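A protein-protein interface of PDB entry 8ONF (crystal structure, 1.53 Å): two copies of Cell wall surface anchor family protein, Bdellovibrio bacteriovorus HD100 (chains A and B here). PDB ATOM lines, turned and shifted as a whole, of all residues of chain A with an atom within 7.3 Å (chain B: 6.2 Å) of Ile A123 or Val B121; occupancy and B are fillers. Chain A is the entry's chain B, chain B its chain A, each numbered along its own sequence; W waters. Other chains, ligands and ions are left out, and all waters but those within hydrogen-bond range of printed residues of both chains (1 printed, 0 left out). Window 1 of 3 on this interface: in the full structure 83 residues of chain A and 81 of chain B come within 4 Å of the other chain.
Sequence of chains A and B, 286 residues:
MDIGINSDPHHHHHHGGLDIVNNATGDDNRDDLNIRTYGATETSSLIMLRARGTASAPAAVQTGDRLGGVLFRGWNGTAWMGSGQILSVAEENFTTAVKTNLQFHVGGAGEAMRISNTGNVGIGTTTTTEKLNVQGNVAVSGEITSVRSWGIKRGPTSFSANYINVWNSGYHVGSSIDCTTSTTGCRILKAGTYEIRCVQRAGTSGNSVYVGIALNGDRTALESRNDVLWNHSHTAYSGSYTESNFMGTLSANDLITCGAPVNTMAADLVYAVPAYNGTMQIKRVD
N of Val B134 sits at hydrogen-bond distance from O of Ala A139 (2.9 Å).
The backbone carbonyl oxygen (O) of Leu B132 is in hydrogen-bond range of the backbone NH (N) of Ala A139 (2.9 Å).
Of the 18 printed residues of chain A, 7 touch a printed residue of chain B.
Of the 17 printed residues of chain B, 8 touch a printed residue of chain A.
Printed residues of chain B that touch a printed residue of chain A: Met B113, Ile B115, Gly B119, Val B121, Lys B131, Leu B132, Asn B133 and Val B134.
Along chain B the printed residues that touch a printed residue of chain A span positions 113 to 134.
The backbone NH (N) of Ile A123 is in hydrogen-bond range of the backbone carbonyl oxygen (O) of Asn A133 (2.9 Å).
O of Asn B133 lies within hydrogen-bond range of N of Ile B123 (2.8 Å).
N of Val B121 sits at hydrogen-bond distance from O of Lys B131 (2.9 Å).
The side-chain amide oxygen of Asn B120 sits at hydrogen-bond distance from the side-chain amino group of Lys B131, at 2.9 Å.
N of Gln A135 is in hydrogen-bond range of O of Ile A123.
The side-chain amino group (NZ) of Lys B131 lies within hydrogen-bond range of the backbone carbonyl oxygen (O) of Thr B118, 3.1 Å away.
Water W1 lies within hydrogen-bond range of the backbone carbonyl oxygen (O) of Gly B119 (2.6 Å), the backbone carbonyl oxygen (O) of Ala A112 (2.8 Å) and the backbone NH (N) of Gly A124 (3.2 Å).
Of the printed residues of chain B, Ala A112 touches Ile B115 and Gly B119.
Ile A123 touches just these residues of chain B: Val B121 (3.7 Å) and Lys B131 (3.7 Å).
Printed residues of chain B within 4 Å of Gly A136: Lys B131.
Of the printed residues of chain A, Met B113 touches Met A113.
Val B121 touches just one residue of chain A: Ile A123.
Printed residues of chain A within 4 Å of Leu B132: Ala A139.
The nearest residue of chain B that does not touch Ile A123 is Leu B132 (4.1 Å).
Met A113 touches its own counterpart, Met B113.
Ile A123 touches Val B121, but with the chains exchanged Val A121 does not touch Ile B123 (8.6 Å).
Positions printed for both chains: 113, 114, 121, 122, 123, 125, 128, 132, 133 and 134.
Among the printed residues, pairs that only touch across the chains: Ala A139 with Asn B133 (3.3 Å), Met A113 with Ile B115 (3.4 Å), Ala A112 with Ile B115 (3.5 Å), Gln A135 with Lys B131 (3.5 Å), Ile A123 with Lys B131 (3.7 Å), Ile A123 with Val B121 (3.7 Å), Val A134 with Lys B131 (3.8 Å), Ala A112 with Gly B119 (3.8 Å), Gly A136 with Lys B131 (3.9 Å) and Met A113 with Met B113 (3.97 Å).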
ATOM      1  N   GLU A 111      26.678  12.250 -24.154  1.00  0.00           N
ATOM      2  CA  GLU A 111      25.307  12.676 -23.924  1.00  0.00           C
ATOM      3  C   GLU A 111      25.008  12.651 -22.426  1.00  0.00           C
ATOM      4  O   GLU A 111      25.208  11.635 -21.750  1.00  0.00           O
ATOM      5  CB  GLU A 111      24.308  11.805 -24.680  1.00  0.00           C
ATOM      6  CG  GLU A 111      22.871  12.311 -24.462  1.00  0.00           C
ATOM      7  CD  GLU A 111      21.791  11.451 -25.105  1.00  0.00           C
ATOM      8  OE1 GLU A 111      22.082  10.705 -26.063  1.00  0.00           O
ATOM      9  OE2 GLU A 111      20.649  11.481 -24.593  1.00  0.00           O
ATOM     10  N   ALA A 112      24.542  13.779 -21.908  1.00  0.00           N
ATOM     11  CA  ALA A 112      24.236  13.921 -20.494  1.00  0.00           C
ATOM     12  C   ALA A 112      22.753  14.017 -20.219  1.00  0.00           C
ATOM     13  O   ALA A 112      22.295  13.546 -19.168  1.00  0.00           O
ATOM     14  CB  ALA A 112      24.917  15.169 -19.914  1.00  0.00           C
ATOM     15  N   MET A 113      21.987  14.614 -21.130  1.00  0.00           N
ATOM     16  CA  MET A 113      20.570  14.796 -20.850  1.00  0.00           C
ATOM     17  C   MET A 113      19.794  14.723 -22.148  1.00  0.00           C
ATOM     18  O   MET A 113      20.243  15.227 -23.178  1.00  0.00           O
ATOM     19  CB  MET A 113      20.303  16.131 -20.140  1.00  0.00           C
ATOM     20  CG  MET A 113      18.835  16.320 -19.783  1.00  0.00           C
ATOM     21  SD  MET A 113      18.593  17.789 -18.758  1.00  0.00           S
ATOM     22  CE  MET A 113      19.775  18.885 -19.516  1.00  0.00           C
ATOM     23  N   ARG A 114      18.653  14.054 -22.103  1.00  0.00           N
ATOM     24  CA  ARG A 114      17.768  13.890 -23.242  1.00  0.00           C
ATOM     25  C   ARG A 114      16.363  14.340 -22.874  1.00  0.00           C
ATOM     26  O   ARG A 114      15.904  14.068 -21.767  1.00  0.00           O
ATOM     27  CB  ARG A 114      17.750  12.428 -23.691  1.00  0.00           C
ATOM     28  CG  ARG A 114      16.704  12.139 -24.704  1.00  0.00           C
ATOM     29  CD  ARG A 114      16.883  10.774 -25.246  1.00  0.00           C
ATOM     30  NE  ARG A 114      18.207  10.569 -25.816  1.00  0.00           N
ATOM     31  CZ  ARG A 114      18.414   9.739 -26.825  1.00  0.00           C
ATOM     32  NH1 ARG A 114      17.411   9.084 -27.377  1.00  0.00           N
ATOM     33  NH2 ARG A 114      19.651   9.549 -27.276  1.00  0.00           N
ATOM     34  N   VAL A 121      12.201  13.504 -19.587  1.00  0.00           N
ATOM     35  CA  VAL A 121      13.594  13.919 -19.458  1.00  0.00           C
ATOM     36  C   VAL A 121      14.405  12.776 -18.863  1.00  0.00           C
ATOM     37  O   VAL A 121      14.020  12.197 -17.840  1.00  0.00           O
ATOM     38  CB  VAL A 121      13.710  15.176 -18.579  1.00  0.00           C
ATOM     39  CG1 VAL A 121      15.181  15.578 -18.341  1.00  0.00           C
ATOM     40  CG2 VAL A 121      12.902  16.331 -19.175  1.00  0.00           C
ATOM     41  N   GLY A 122      15.544  12.477 -19.478  1.00  0.00           N
ATOM     42  CA  GLY A 122      16.510  11.536 -18.934  1.00  0.00           C
ATOM     43  C   GLY A 122      17.828  12.212 -18.618  1.00  0.00           C
ATOM     44  O   GLY A 122      18.366  12.953 -19.447  1.00  0.00           O
ATOM     45  N   ILE A 123      18.357  11.976 -17.428  1.00  0.00           N
ATOM     46  CA  ILE A 123      19.673  12.459 -17.022  1.00  0.00           C
ATOM     47  C   ILE A 123      20.507  11.220 -16.743  1.00  0.00           C
ATOM     48  O   ILE A 123      20.221  10.482 -15.787  1.00  0.00           O
ATOM     49  CB  ILE A 123      19.606  13.366 -15.783  1.00  0.00           C
ATOM     50  CG1 ILE A 123      18.724  14.599 -16.058  1.00  0.00           C
ATOM     51  CG2 ILE A 123      21.013  13.787 -15.357  1.00  0.00           C
ATOM     52  CD1 ILE A 123      18.475  15.493 -14.854  1.00  0.00           C
ATOM     53  N   GLY A 124      21.519  10.976 -17.574  1.00  0.00           N
ATOM     54  CA  GLY A 124      22.332   9.782 -17.457  1.00  0.00           C
ATOM     55  C   GLY A 124      21.725   8.541 -18.069  1.00  0.00           C
ATOM     56  O   GLY A 124      22.319   7.460 -17.953  1.00  0.00           O
ATOM     57  N   THR A 125      20.575   8.672 -18.733  1.00  0.00           N
ATOM     58  CA  THR A 125      19.896   7.573 -19.406  1.00  0.00           C
ATOM     59  C   THR A 125      19.167   8.123 -20.625  1.00  0.00           C
ATOM     60  O   THR A 125      18.725   9.280 -20.629  1.00  0.00           O
ATOM     61  CB  THR A 125      18.898   6.856 -18.478  1.00  0.00           C
ATOM     62  OG1 THR A 125      18.258   5.797 -19.194  1.00  0.00           O
ATOM     63  CG2 THR A 125      17.830   7.836 -17.982  1.00  0.00           C
ATOM     64  N   THR A 126      19.028   7.283 -21.650  1.00  0.00           N
ATOM     65  CA  THR A 126      18.177   7.607 -22.785  1.00  0.00           C
ATOM     66  C   THR A 126      16.809   6.948 -22.688  1.00  0.00           C
ATOM     67  O   THR A 126      15.968   7.160 -23.569  1.00  0.00           O
ATOM     68  CB  THR A 126      18.848   7.199 -24.103  1.00  0.00           C
ATOM     69  OG1 THR A 126      19.017   5.777 -24.141  1.00  0.00           O
ATOM     70  CG2 THR A 126      20.215   7.880 -24.239  1.00  0.00           C
ATOM     71  N   THR A 127      16.568   6.145 -21.653  1.00  0.00           N
ATOM     72  CA  THR A 127      15.283   5.471 -21.474  1.00  0.00           C
ATOM     73  C   THR A 127      14.422   6.389 -20.614  1.00  0.00           C
ATOM     74  O   THR A 127      14.616   6.485 -19.399  1.00  0.00           O
ATOM     75  CB  THR A 127      15.478   4.094 -20.846  1.00  0.00           C
ATOM     76  OG1 THR A 127      16.275   3.284 -21.722  1.00  0.00           O
ATOM     77  CG2 THR A 127      14.138   3.402 -20.643  1.00  0.00           C
ATOM     78  N   THR A 128      13.476   7.087 -21.252  1.00  0.00           N
ATOM     79  CA  THR A 128      12.736   8.156 -20.582  1.00  0.00           C
ATOM     80  C   THR A 128      11.315   7.722 -20.233  1.00  0.00           C
ATOM     81  O   THR A 128      10.333   8.271 -20.752  1.00  0.00           O
ATOM     82  CB  THR A 128      12.733   9.421 -21.466  1.00  0.00           C
ATOM     83  OG1 THR A 128      12.170   9.127 -22.756  1.00  0.00           O
ATOM     84  CG2 THR A 128      14.162   9.948 -21.643  1.00  0.00           C
ATOM     85  N   LEU A 132      10.598  12.484 -15.352  1.00  0.00           N
ATOM     86  CA  LEU A 132      12.014  12.684 -15.067  1.00  0.00           C
ATOM     87  C   LEU A 132      12.616  11.352 -14.657  1.00  0.00           C
ATOM     88  O   LEU A 132      12.042  10.645 -13.827  1.00  0.00           O
ATOM     89  CB  LEU A 132      12.245  13.747 -13.974  1.00  0.00           C
ATOM     90  CG  LEU A 132      13.705  13.986 -13.558  1.00  0.00           C
ATOM     91  CD1 LEU A 132      14.581  14.511 -14.701  1.00  0.00           C
ATOM     92  CD2 LEU A 132      13.785  14.959 -12.368  1.00  0.00           C
ATOM     93  N   ASN A 133      13.751  11.003 -15.264  1.00  0.00           N
ATOM     94  CA  ASN A 133      14.470   9.762 -14.988  1.00  0.00           C
ATOM     95  C   ASN A 133      15.933  10.094 -14.745  1.00  0.00           C
ATOM     96  O   ASN A 133      16.552  10.765 -15.576  1.00  0.00           O
ATOM     97  CB  ASN A 133      14.351   8.789 -16.161  1.00  0.00           C
ATOM     98  CG  ASN A 133      12.946   8.687 -16.678  1.00  0.00           C
ATOM     99  OD1 ASN A 133      12.205   7.768 -16.311  1.00  0.00           O
ATOM    100  ND2 ASN A 133      12.559   9.617 -17.561  1.00  0.00           N
ATOM    101  N   VAL A 134      16.480   9.665 -13.610  1.00  0.00           N
ATOM    102  CA  VAL A 134      17.864   9.965 -13.247  1.00  0.00           C
ATOM    103  C   VAL A 134      18.593   8.654 -13.013  1.00  0.00           C
ATOM    104  O   VAL A 134      18.197   7.863 -12.149  1.00  0.00           O
ATOM    105  CB  VAL A 134      17.954  10.849 -11.993  1.00  0.00           C
ATOM    106  CG1 VAL A 134      19.413  11.158 -11.675  1.00  0.00           C
ATOM    107  CG2 VAL A 134      17.139  12.136 -12.176  1.00  0.00           C
ATOM    108  N   GLN A 135      19.672   8.437 -13.752  1.00  0.00           N
ATOM    109  CA  GLN A 135      20.471   7.219 -13.626  1.00  0.00           C
ATOM    110  C   GLN A 135      21.657   7.591 -12.740  1.00  0.00           C
ATOM    111  O   GLN A 135      22.724   8.004 -13.205  1.00  0.00           O
ATOM    112  CB  GLN A 135      20.894   6.717 -15.008  1.00  0.00           C
ATOM    113  CG  GLN A 135      21.651   5.397 -15.032  1.00  0.00           C
ATOM    114  CD  GLN A 135      20.822   4.227 -14.524  1.00  0.00           C
ATOM    115  OE1 GLN A 135      19.608   4.173 -14.747  1.00  0.00           O
ATOM    116  NE2 GLN A 135      21.479   3.259 -13.882  1.00  0.00           N
ATOM    117  N   GLY A 136      21.445   7.465 -11.438  1.00  0.00           N
ATOM    118  CA  GLY A 136      22.380   7.917 -10.436  1.00  0.00           C
ATOM    119  C   GLY A 136      21.614   8.323  -9.190  1.00  0.00           C
ATOM    120  O   GLY A 136      20.451   7.958  -9.018  1.00  0.00           O
ATOM    121  N   ALA A 139      20.639  14.665  -5.051  1.00  0.00           N
ATOM    122  CA  ALA A 139      20.877  15.388  -3.806  1.00  0.00           C
ATOM    123  C   ALA A 139      20.078  16.681  -3.827  1.00  0.00           C
ATOM    124  O   ALA A 139      20.248  17.505  -4.729  1.00  0.00           O
ATOM    125  CB  ALA A 139      22.363  15.697  -3.614  1.00  0.00           C
ATOM    126  N   MET B 113      21.421  26.529 -14.524  1.00  0.00           N
ATOM    127  CA  MET B 113      21.634  25.091 -14.595  1.00  0.00           C
ATOM    128  C   MET B 113      23.002  24.826 -15.200  1.00  0.00           C
ATOM    129  O   MET B 113      23.422  25.515 -16.129  1.00  0.00           O
ATOM    130  CB  MET B 113      20.536  24.405 -15.422  1.00  0.00           C
ATOM    131  CG  MET B 113      20.697  22.905 -15.575  1.00  0.00           C
ATOM    132  SD  MET B 113      19.158  22.107 -16.113  1.00  0.00           S
ATOM    133  CE  MET B 113      19.238  22.453 -17.857  1.00  0.00           C
ATOM    134  N   ARG B 114      23.690  23.836 -14.657  1.00  0.00           N
ATOM    135  CA  ARG B 114      25.014  23.434 -15.091  1.00  0.00           C
ATOM    136  C   ARG B 114      25.006  21.950 -15.405  1.00  0.00           C
ATOM    137  O   ARG B 114      24.432  21.173 -14.648  1.00  0.00           O
ATOM    138  CB  ARG B 114      26.042  23.722 -13.986  1.00  0.00           C
ATOM    139  CG  ARG B 114      27.337  23.080 -14.291  1.00  0.00           C
ATOM    140  CD  ARG B 114      28.444  23.733 -13.586  1.00  0.00           C
ATOM    141  NE  ARG B 114      28.527  25.165 -13.852  1.00  0.00           N
ATOM    142  CZ  ARG B 114      29.661  25.835 -13.734  1.00  0.00           C
ATOM    143  NH1 ARG B 114      30.807  25.202 -13.556  1.00  0.00           N
ATOM    144  NH2 ARG B 114      29.645  27.166 -13.771  1.00  0.00           N
ATOM    145  N   ILE B 115      25.667  21.551 -16.487  1.00  0.00           N
ATOM    146  CA  ILE B 115      25.943  20.147 -16.776  1.00  0.00           C
ATOM    147  C   ILE B 115      27.455  19.999 -16.826  1.00  0.00           C
ATOM    148  O   ILE B 115      28.107  20.578 -17.704  1.00  0.00           O
ATOM    149  CB  ILE B 115      25.318  19.674 -18.098  1.00  0.00           C
ATOM    150  CG1 ILE B 115      23.827  19.969 -18.148  1.00  0.00           C
ATOM    151  CG2 ILE B 115      25.620  18.180 -18.309  1.00  0.00           C
ATOM    152  CD1 ILE B 115      23.156  19.524 -19.463  1.00  0.00           C
ATOM    153  N   SER B 116      28.017  19.229 -15.899  1.00  0.00           N
ATOM    154  CA  SER B 116      29.464  19.099 -15.807  1.00  0.00           C
ATOM    155  C   SER B 116      29.967  18.002 -16.744  1.00  0.00           C
ATOM    156  O   SER B 116      29.194  17.260 -17.350  1.00  0.00           O
ATOM    157  CB  SER B 116      29.884  18.804 -14.367  1.00  0.00           C
ATOM    158  OG  SER B 116      29.529  19.880 -13.514  1.00  0.00           O
ATOM    159  N   THR B 118      31.206  15.246 -16.197  1.00  0.00           N
ATOM    160  CA  THR B 118      30.744  13.962 -15.692  1.00  0.00           C
ATOM    161  C   THR B 118      29.322  13.620 -16.116  1.00  0.00           C
ATOM    162  O   THR B 118      28.859  12.508 -15.823  1.00  0.00           O
ATOM    163  CB  THR B 118      30.787  14.018 -14.177  1.00  0.00           C
ATOM    164  OG1 THR B 118      29.962  15.117 -13.775  1.00  0.00           O
ATOM    165  CG2 THR B 118      32.199  14.233 -13.674  1.00  0.00           C
ATOM    166  N   GLY B 119      28.616  14.543 -16.770  1.00  0.00           N
ATOM    167  CA  GLY B 119      27.192  14.397 -16.988  1.00  0.00           C
ATOM    168  C   GLY B 119      26.334  14.838 -15.820  1.00  0.00           C
ATOM    169  O   GLY B 119      25.103  14.863 -15.943  1.00  0.00           O
ATOM    170  N   ASN B 120      26.939  15.203 -14.698  1.00  0.00           N
ATOM    171  CA  ASN B 120      26.163  15.545 -13.510  1.00  0.00           C
ATOM    172  C   ASN B 120      25.544  16.926 -13.670  1.00  0.00           C
ATOM    173  O   ASN B 120      26.190  17.855 -14.162  1.00  0.00           O
ATOM    174  CB  ASN B 120      27.045  15.503 -12.265  1.00  0.00           C
ATOM    175  CG  ASN B 120      27.498  14.090 -11.908  1.00  0.00           C
ATOM    176  OD1 ASN B 120      27.150  13.108 -12.579  1.00  0.00           O
ATOM    177  ND2 ASN B 120      28.276  13.982 -10.838  1.00  0.00           N
ATOM    178  N   VAL B 121      24.284  17.056 -13.257  1.00  0.00           N
ATOM    179  CA  VAL B 121      23.495  18.261 -13.470  1.00  0.00           C
ATOM    180  C   VAL B 121      23.300  18.978 -12.143  1.00  0.00           C
ATOM    181  O   VAL B 121      22.949  18.348 -11.142  1.00  0.00           O
ATOM    182  CB  VAL B 121      22.139  17.920 -14.105  1.00  0.00           C
ATOM    183  CG1 VAL B 121      21.273  19.185 -14.237  1.00  0.00           C
ATOM    184  CG2 VAL B 121      22.358  17.252 -15.444  1.00  0.00           C
ATOM    185  N   GLY B 122      23.494  20.297 -12.142  1.00  0.00           N
ATOM    186  CA  GLY B 122      23.188  21.114 -10.985  1.00  0.00           C
ATOM    187  C   GLY B 122      22.157  22.161 -11.336  1.00  0.00           C
ATOM    188  O   GLY B 122      22.276  22.831 -12.366  1.00  0.00           O
ATOM    189  N   ILE B 123      21.128  22.296 -10.509  1.00  0.00           N
ATOM    190  CA  ILE B 123      20.103  23.318 -10.649  1.00  0.00           C
ATOM    191  C   ILE B 123      20.232  24.199  -9.426  1.00  0.00           C
ATOM    192  O   ILE B 123      19.939  23.752  -8.308  1.00  0.00           O
ATOM    193  CB  ILE B 123      18.695  22.725 -10.752  1.00  0.00           C
ATOM    194  CG1 ILE B 123      18.601  21.787 -11.965  1.00  0.00           C
ATOM    195  CG2 ILE B 123      17.673  23.848 -10.860  1.00  0.00           C
ATOM    196  CD1 ILE B 123      17.214  21.128 -12.135  1.00  0.00           C
ATOM    197  N   THR B 125      23.101  25.174  -8.308  1.00  0.00           N
ATOM    198  CA  THR B 125      24.443  24.957  -7.791  1.00  0.00           C
ATOM    199  C   THR B 125      25.372  24.644  -8.953  1.00  0.00           C
ATOM    200  O   THR B 125      24.949  24.079  -9.966  1.00  0.00           O
ATOM    201  CB  THR B 125      24.502  23.814  -6.754  1.00  0.00           C
ATOM    202  OG1 THR B 125      25.860  23.640  -6.317  1.00  0.00           O
ATOM    203  CG2 THR B 125      23.988  22.505  -7.337  1.00  0.00           C
ATOM    204  N   THR B 128      28.418  19.851  -8.747  1.00  0.00           N
ATOM    205  CA  THR B 128      27.546  18.779  -9.229  1.00  0.00           C
ATOM    206  C   THR B 128      28.021  17.430  -8.684  1.00  0.00           C
ATOM    207  O   THR B 128      28.529  16.579  -9.400  1.00  0.00           O
ATOM    208  CB  THR B 128      27.523  18.776 -10.757  1.00  0.00           C
ATOM    209  OG1 THR B 128      28.858  18.656 -11.252  1.00  0.00           O
ATOM    210  CG2 THR B 128      26.947  20.095 -11.288  1.00  0.00           C
ATOM    211  N   GLU B 130      26.353  14.782  -7.241  1.00  0.00           N
ATOM    212  CA  GLU B 130      25.595  13.619  -7.693  1.00  0.00           C
ATOM    213  C   GLU B 130      25.073  13.850  -9.114  1.00  0.00           C
ATOM    214  O   GLU B 130      25.243  14.923  -9.699  1.00  0.00           O
ATOM    215  CB  GLU B 130      24.447  13.301  -6.730  1.00  0.00           C
ATOM    216  CG  GLU B 130      24.881  12.994  -5.289  1.00  0.00           C
ATOM    217  CD  GLU B 130      25.739  11.732  -5.153  1.00  0.00           C
ATOM    218  OE1 GLU B 130      25.804  10.925  -6.099  1.00  0.00           O
ATOM    219  OE2 GLU B 130      26.353  11.553  -4.079  1.00  0.00           O
ATOM    220  N   LYS B 131      24.418  12.825  -9.675  1.00  0.00           N
ATOM    221  CA  LYS B 131      23.923  12.921 -11.050  1.00  0.00           C
ATOM    222  C   LYS B 131      22.935  14.069 -11.218  1.00  0.00           C
ATOM    223  O   LYS B 131      22.878  14.689 -12.287  1.00  0.00           O
ATOM    224  CB  LYS B 131      23.271  11.602 -11.466  1.00  0.00           C
ATOM    225  CG  LYS B 131      22.937  11.489 -12.952  1.00  0.00           C
ATOM    226  CD  LYS B 131      24.163  11.771 -13.827  1.00  0.00           C
ATOM    227  CE  LYS B 131      25.211  10.689 -13.688  1.00  0.00           C
ATOM    228  NZ  LYS B 131      26.470  11.035 -14.436  1.00  0.00           N
ATOM    229  N   LEU B 132      22.136  14.350 -10.193  1.00  0.00           N
ATOM    230  CA  LEU B 132      21.288  15.537 -10.167  1.00  0.00           C
ATOM    231  C   LEU B 132      21.400  16.184  -8.796  1.00  0.00           C
ATOM    232  O   LEU B 132      21.362  15.490  -7.779  1.00  0.00           O
ATOM    233  CB  LEU B 132      19.826  15.179 -10.473  1.00  0.00           C
ATOM    234  CG  LEU B 132      18.844  16.348 -10.405  1.00  0.00           C
ATOM    235  CD1 LEU B 132      19.257  17.455 -11.382  1.00  0.00           C
ATOM    236  CD2 LEU B 132      17.405  15.891 -10.658  1.00  0.00           C
ATOM    237  N   ASN B 133      21.571  17.505  -8.768  1.00  0.00           N
ATOM    238  CA  ASN B 133      21.705  18.276  -7.546  1.00  0.00           C
ATOM    239  C   ASN B 133      20.761  19.458  -7.648  1.00  0.00           C
ATOM    240  O   ASN B 133      20.766  20.159  -8.665  1.00  0.00           O
ATOM    241  CB  ASN B 133      23.149  18.759  -7.369  1.00  0.00           C
ATOM    242  CG  ASN B 133      24.173  17.651  -7.600  1.00  0.00           C
ATOM    243  OD1 ASN B 133      24.607  16.991  -6.655  1.00  0.00           O
ATOM    244  ND2 ASN B 133      24.527  17.419  -8.864  1.00  0.00           N
ATOM    245  N   VAL B 134      19.950  19.677  -6.616  1.00  0.00           N
ATOM    246  CA  VAL B 134      18.976  20.763  -6.592  1.00  0.00           C
ATOM    247  C   VAL B 134      19.220  21.582  -5.340  1.00  0.00           C
ATOM    248  O   VAL B 134      19.092  21.067  -4.223  1.00  0.00           O
ATOM    249  CB  VAL B 134      17.525  20.258  -6.619  1.00  0.00           C
ATOM    250  CG1 VAL B 134      16.548  21.443  -6.619  1.00  0.00           C
ATOM    251  CG2 VAL B 134      17.298  19.367  -7.838  1.00  0.00           C
HETATM  252  O   HOH W   1      24.177  12.778 -17.281  1.00  0.00           O
